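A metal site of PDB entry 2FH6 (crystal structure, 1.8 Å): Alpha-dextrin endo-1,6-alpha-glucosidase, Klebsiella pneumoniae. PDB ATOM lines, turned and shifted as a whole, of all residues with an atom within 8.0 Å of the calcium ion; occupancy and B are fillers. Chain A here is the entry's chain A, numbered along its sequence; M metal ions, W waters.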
ATOM      1  N   THR A 484      16.922  29.673  29.737  1.00  0.00           N
ATOM      2  CA  THR A 484      16.383  29.105  28.507  1.00  0.00           C
ATOM      3  C   THR A 484      17.273  28.749  27.324  1.00  0.00           C
ATOM      4  O   THR A 484      16.773  28.547  26.214  1.00  0.00           O
ATOM      5  CB  THR A 484      15.221  29.966  28.033  1.00  0.00           C
ATOM      6  OG1 THR A 484      15.613  31.342  28.052  1.00  0.00           O
ATOM      7  CG2 THR A 484      14.017  29.782  28.951  1.00  0.00           C
ATOM      8  N   VAL A 485      18.577  28.655  27.552  1.00  0.00           N
ATOM      9  CA  VAL A 485      19.506  28.240  26.514  1.00  0.00           C
ATOM     10  C   VAL A 485      20.446  27.256  27.217  1.00  0.00           C
ATOM     11  O   VAL A 485      21.001  27.568  28.267  1.00  0.00           O
ATOM     12  CB  VAL A 485      20.335  29.416  25.945  1.00  0.00           C
ATOM     13  CG1 VAL A 485      21.440  28.880  25.038  1.00  0.00           C
ATOM     14  CG2 VAL A 485      19.415  30.338  25.123  1.00  0.00           C
ATOM     15  N   ASN A 486      20.597  26.060  26.651  1.00  0.00           N
ATOM     16  CA  ASN A 486      21.474  25.063  27.261  1.00  0.00           C
ATOM     17  C   ASN A 486      22.918  25.493  26.996  1.00  0.00           C
ATOM     18  O   ASN A 486      23.303  25.704  25.837  1.00  0.00           O
ATOM     19  CB  ASN A 486      21.208  23.676  26.668  1.00  0.00           C
ATOM     20  CG  ASN A 486      21.825  22.576  27.511  1.00  0.00           C
ATOM     21  OD1 ASN A 486      22.961  22.690  27.976  1.00  0.00           O
ATOM     22  ND2 ASN A 486      21.085  21.487  27.700  1.00  0.00           N
ATOM     23  N   ASP A 494      22.333  24.794  16.011  1.00  0.00           N
ATOM     24  CA  ASP A 494      21.906  26.056  15.432  1.00  0.00           C
ATOM     25  C   ASP A 494      21.690  25.912  13.934  1.00  0.00           C
ATOM     26  O   ASP A 494      22.154  24.939  13.326  1.00  0.00           O
ATOM     27  CB  ASP A 494      22.925  27.149  15.762  1.00  0.00           C
ATOM     28  CG  ASP A 494      22.840  27.589  17.210  1.00  0.00           C
ATOM     29  OD1 ASP A 494      21.764  28.092  17.596  1.00  0.00           O
ATOM     30  OD2 ASP A 494      23.817  27.421  17.967  1.00  0.00           O
ATOM     31  N   ASN A 546      10.997  25.847  12.209  1.00  0.00           N
ATOM     32  CA  ASN A 546      11.678  26.716  13.148  1.00  0.00           C
ATOM     33  C   ASN A 546      11.193  26.539  14.579  1.00  0.00           C
ATOM     34  O   ASN A 546      11.991  26.615  15.513  1.00  0.00           O
ATOM     35  CB  ASN A 546      11.527  28.177  12.734  1.00  0.00           C
ATOM     36  CG  ASN A 546      12.596  29.059  13.351  1.00  0.00           C
ATOM     37  OD1 ASN A 546      13.784  28.801  13.182  1.00  0.00           O
ATOM     38  ND2 ASN A 546      12.182  30.098  14.064  1.00  0.00           N
ATOM     39  N   THR A 547       9.899  26.307  14.760  1.00  0.00           N
ATOM     40  CA  THR A 547       9.337  26.117  16.089  1.00  0.00           C
ATOM     41  C   THR A 547      10.034  24.945  16.786  1.00  0.00           C
ATOM     42  O   THR A 547      10.228  24.964  17.994  1.00  0.00           O
ATOM     43  CB  THR A 547       7.812  25.866  16.022  1.00  0.00           C
ATOM     44  OG1 THR A 547       7.166  27.043  15.498  1.00  0.00           O
ATOM     45  CG2 THR A 547       7.245  25.573  17.399  1.00  0.00           C
ATOM     46  N   LEU A 548      10.422  23.940  16.003  1.00  0.00           N
ATOM     47  CA  LEU A 548      11.111  22.766  16.556  1.00  0.00           C
ATOM     48  C   LEU A 548      12.579  23.123  16.804  1.00  0.00           C
ATOM     49  O   LEU A 548      13.172  22.701  17.805  1.00  0.00           O
ATOM     50  CB  LEU A 548      11.021  21.582  15.588  1.00  0.00           C
ATOM     51  CG  LEU A 548       9.600  21.135  15.237  1.00  0.00           C
ATOM     52  CD1 LEU A 548       9.665  19.931  14.310  1.00  0.00           C
ATOM     53  CD2 LEU A 548       8.829  20.795  16.506  1.00  0.00           C
ATOM     54  N   VAL A 549      13.156  23.883  15.886  1.00  0.00           N
ATOM     55  CA  VAL A 549      14.555  24.302  16.002  1.00  0.00           C
ATOM     56  C   VAL A 549      14.756  25.136  17.269  1.00  0.00           C
ATOM     57  O   VAL A 549      15.773  25.016  17.963  1.00  0.00           O
ATOM     58  CB  VAL A 549      14.973  25.184  14.790  1.00  0.00           C
ATOM     59  CG1 VAL A 549      16.383  25.722  15.006  1.00  0.00           C
ATOM     60  CG2 VAL A 549      14.897  24.354  13.502  1.00  0.00           C
ATOM     61  N   ALA A 550      13.762  25.980  17.567  1.00  0.00           N
ATOM     62  CA  ALA A 550      13.818  26.862  18.724  1.00  0.00           C
ATOM     63  C   ALA A 550      14.032  26.171  20.066  1.00  0.00           C
ATOM     64  O   ALA A 550      14.610  26.758  20.996  1.00  0.00           O
ATOM     65  CB  ALA A 550      12.537  27.696  18.776  1.00  0.00           C
ATOM     66  N   GLN A 551      13.591  24.924  20.174  1.00  0.00           N
ATOM     67  CA  GLN A 551      13.693  24.145  21.409  1.00  0.00           C
ATOM     68  C   GLN A 551      15.127  23.818  21.816  1.00  0.00           C
ATOM     69  O   GLN A 551      15.427  23.687  23.003  1.00  0.00           O
ATOM     70  CB  GLN A 551      12.914  22.833  21.268  1.00  0.00           C
ATOM     71  CG  GLN A 551      11.453  22.998  20.916  1.00  0.00           C
ATOM     72  CD  GLN A 551      10.815  21.692  20.469  1.00  0.00           C
ATOM     73  OE1 GLN A 551       9.591  21.614  20.311  1.00  0.00           O
ATOM     74  NE2 GLN A 551      11.638  20.677  20.254  1.00  0.00           N
ATOM     75  N   THR A 552      16.005  23.692  20.830  1.00  0.00           N
ATOM     76  CA  THR A 552      17.378  23.308  21.115  1.00  0.00           C
ATOM     77  C   THR A 552      18.459  24.188  20.493  1.00  0.00           C
ATOM     78  O   THR A 552      19.599  23.739  20.330  1.00  0.00           O
ATOM     79  CB  THR A 552      17.605  21.844  20.675  1.00  0.00           C
ATOM     80  OG1 THR A 552      17.101  21.651  19.351  1.00  0.00           O
ATOM     81  CG2 THR A 552      16.878  20.887  21.616  1.00  0.00           C
ATOM     82  N   ASP A 553      18.127  25.427  20.150  1.00  0.00           N
ATOM     83  CA  ASP A 553      19.131  26.316  19.570  1.00  0.00           C
ATOM     84  C   ASP A 553      19.762  27.196  20.656  1.00  0.00           C
ATOM     85  O   ASP A 553      19.500  27.020  21.846  1.00  0.00           O
ATOM     86  CB  ASP A 553      18.529  27.191  18.451  1.00  0.00           C
ATOM     87  CG  ASP A 553      17.398  28.084  18.931  1.00  0.00           C
ATOM     88  OD1 ASP A 553      17.204  28.227  20.159  1.00  0.00           O
ATOM     89  OD2 ASP A 553      16.702  28.678  18.070  1.00  0.00           O
ATOM     90  N   SER A 554      20.596  28.141  20.234  1.00  0.00           N
ATOM     91  CA  SER A 554      21.275  29.029  21.185  1.00  0.00           C
ATOM     92  C   SER A 554      20.515  30.329  21.365  1.00  0.00           C
ATOM     93  O   SER A 554      21.009  31.262  22.006  1.00  0.00           O
ATOM     94  CB  SER A 554      22.680  29.359  20.664  1.00  0.00           C
ATOM     95  OG  SER A 554      23.457  28.194  20.499  1.00  0.00           O
ATOM     96  N   TYR A 555      19.295  30.399  20.834  1.00  0.00           N
ATOM     97  CA  TYR A 555      18.523  31.631  20.891  1.00  0.00           C
ATOM     98  C   TYR A 555      17.364  31.792  21.869  1.00  0.00           C
ATOM     99  O   TYR A 555      16.522  30.907  22.018  1.00  0.00           O
ATOM    100  CB  TYR A 555      17.981  31.944  19.479  1.00  0.00           C
ATOM    101  CG  TYR A 555      17.521  33.382  19.323  1.00  0.00           C
ATOM    102  CD1 TYR A 555      16.332  33.828  19.925  1.00  0.00           C
ATOM    103  CD2 TYR A 555      18.304  34.304  18.655  1.00  0.00           C
ATOM    104  CE1 TYR A 555      15.971  35.173  19.867  1.00  0.00           C
ATOM    105  CE2 TYR A 555      17.951  35.647  18.585  1.00  0.00           C
ATOM    106  CZ  TYR A 555      16.784  36.072  19.198  1.00  0.00           C
ATOM    107  OH  TYR A 555      16.446  37.408  19.167  1.00  0.00           O
ATOM    108  N   ASN A 556      17.339  32.960  22.510  1.00  0.00           N
ATOM    109  CA  ASN A 556      16.286  33.371  23.421  1.00  0.00           C
ATOM    110  C   ASN A 556      16.603  34.771  23.925  1.00  0.00           C
ATOM    111  O   ASN A 556      17.770  35.103  24.148  1.00  0.00           O
ATOM    112  CB  ASN A 556      16.148  32.423  24.613  1.00  0.00           C
ATOM    113  CG  ASN A 556      14.791  32.531  25.278  1.00  0.00           C
ATOM    114  OD1 ASN A 556      14.451  33.568  25.859  1.00  0.00           O
ATOM    115  ND2 ASN A 556      13.988  31.473  25.173  1.00  0.00           N
ATOM    116  N   TRP A 557      15.575  35.603  24.088  1.00  0.00           N
ATOM    117  CA  TRP A 557      15.807  36.941  24.609  1.00  0.00           C
ATOM    118  C   TRP A 557      16.451  36.830  25.988  1.00  0.00           C
ATOM    119  O   TRP A 557      17.307  37.639  26.356  1.00  0.00           O
ATOM    120  CB  TRP A 557      14.505  37.721  24.739  1.00  0.00           C
ATOM    121  CG  TRP A 557      13.956  38.239  23.456  1.00  0.00           C
ATOM    122  CD1 TRP A 557      14.598  38.337  22.264  1.00  0.00           C
ATOM    123  CD2 TRP A 557      12.637  38.751  23.247  1.00  0.00           C
ATOM    124  NE1 TRP A 557      13.763  38.873  21.305  1.00  0.00           N
ATOM    125  CE2 TRP A 557      12.548  39.137  21.889  1.00  0.00           C
ATOM    126  CE3 TRP A 557      11.510  38.914  24.072  1.00  0.00           C
ATOM    127  CZ2 TRP A 557      11.383  39.681  21.341  1.00  0.00           C
ATOM    128  CZ3 TRP A 557      10.349  39.449  23.529  1.00  0.00           C
ATOM    129  CH2 TRP A 557      10.295  39.829  22.171  1.00  0.00           C
ATOM    130  N   SER A 891       8.938  37.672  19.245  1.00  0.00           N
ATOM    131  CA  SER A 891      10.024  36.839  18.755  1.00  0.00           C
ATOM    132  C   SER A 891      11.044  36.279  19.741  1.00  0.00           C
ATOM    133  O   SER A 891      12.096  35.802  19.315  1.00  0.00           O
ATOM    134  CB  SER A 891      10.780  37.602  17.662  1.00  0.00           C
ATOM    135  OG  SER A 891      11.544  38.665  18.210  1.00  0.00           O
ATOM    136  N   TYR A 892      10.733  36.305  21.031  1.00  0.00           N
ATOM    137  CA  TYR A 892      11.654  35.842  22.074  1.00  0.00           C
ATOM    138  C   TYR A 892      12.292  34.470  21.864  1.00  0.00           C
ATOM    139  O   TYR A 892      13.401  34.231  22.344  1.00  0.00           O
ATOM    140  CB  TYR A 892      10.962  35.828  23.447  1.00  0.00           C
ATOM    141  CG  TYR A 892      10.081  34.619  23.692  1.00  0.00           C
ATOM    142  CD1 TYR A 892       8.864  34.450  23.020  1.00  0.00           C
ATOM    143  CD2 TYR A 892      10.466  33.628  24.603  1.00  0.00           C
ATOM    144  CE1 TYR A 892       8.058  33.336  23.249  1.00  0.00           C
ATOM    145  CE2 TYR A 892       9.665  32.512  24.845  1.00  0.00           C
ATOM    146  CZ  TYR A 892       8.459  32.370  24.165  1.00  0.00           C
ATOM    147  OH  TYR A 892       7.667  31.276  24.390  1.00  0.00           O
ATOM    148  N   ASP A 893      11.599  33.580  21.174  1.00  0.00           N
ATOM    149  CA  ASP A 893      12.115  32.222  20.947  1.00  0.00           C
ATOM    150  C   ASP A 893      12.029  31.864  19.468  1.00  0.00           C
ATOM    151  O   ASP A 893      12.015  30.678  19.128  1.00  0.00           O
ATOM    152  CB  ASP A 893      11.290  31.234  21.778  1.00  0.00           C
ATOM    153  CG  ASP A 893      11.991  29.911  21.991  1.00  0.00           C
ATOM    154  OD1 ASP A 893      11.312  28.946  22.392  1.00  0.00           O
ATOM    155  OD2 ASP A 893      13.221  29.829  21.756  1.00  0.00           O
ATOM    156  N   SER A 894      11.981  32.878  18.613  1.00  0.00           N
ATOM    157  CA  SER A 894      11.875  32.663  17.173  1.00  0.00           C
ATOM    158  C   SER A 894      13.208  32.473  16.459  1.00  0.00           C
ATOM    159  O   SER A 894      13.265  32.472  15.225  1.00  0.00           O
ATOM    160  CB  SER A 894      11.084  33.801  16.525  1.00  0.00           C
ATOM    161  OG  SER A 894       9.723  33.720  16.929  1.00  0.00           O
ATOM    162  N   GLY A 895      14.270  32.316  17.244  1.00  0.00           N
ATOM    163  CA  GLY A 895      15.603  32.057  16.712  1.00  0.00           C
ATOM    164  C   GLY A 895      16.298  33.063  15.815  1.00  0.00           C
ATOM    165  O   GLY A 895      15.856  34.192  15.625  1.00  0.00           O
ATOM    166  N   ASP A 896      17.433  32.630  15.261  1.00  0.00           N
ATOM    167  CA  ASP A 896      18.232  33.444  14.360  1.00  0.00           C
ATOM    168  C   ASP A 896      17.453  33.795  13.092  1.00  0.00           C
ATOM    169  O   ASP A 896      17.655  34.850  12.502  1.00  0.00           O
ATOM    170  CB  ASP A 896      19.508  32.713  13.931  1.00  0.00           C
ATOM    171  CG  ASP A 896      20.486  32.493  15.066  1.00  0.00           C
ATOM    172  OD1 ASP A 896      20.450  33.262  16.058  1.00  0.00           O
ATOM    173  OD2 ASP A 896      21.303  31.553  14.960  1.00  0.00           O
HETATM  174 CA    CA M   1      15.426  28.938  21.656  1.00  0.00          CA
HETATM  175  O   HOH W   1      14.874  29.956  19.439  1.00  0.00           O
HETATM  176  O   HOH W   2      17.114  27.774  22.876  1.00  0.00           O
HETATM  177  O   HOH W   3      14.884  28.942  24.086  1.00  0.00           O
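Water W2 lies within hydrogen-bond range of the backbone carbonyl oxygen of Asp 553 and the backbone carbonyl oxygen of Thr 484. Water W3 bridges O of Thr 484 and ND2 of Asn 556. Water W1 lies within hydrogen-bond range of the side-chain carboxylate of Asp 553, the backbone carbonyl oxygen of Asp 893 and the backbone NH of Gly 895.
The calcium ion is bound by the backbone carbonyl oxygen (O) of Tyr 555 (2.3 Å), the side-chain carboxylate (OD2) of Asp 893 (2.4 Å), water W2 (2.4 Å), the backbone carbonyl oxygen (O) of Ala 550 (2.4 Å), the side-chain carboxylate (OD1) of Asp 553 (2.4 Å), water W3 (2.5 Å) and water W1 (2.5 Å).
Four residues have an atom within 4 Å of the calcium ion: Ala 550, Asp 553, Tyr 555 and Asp 893. The nearest printed residue that does not touch the calcium ion is Asn 556 (4.5 Å).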
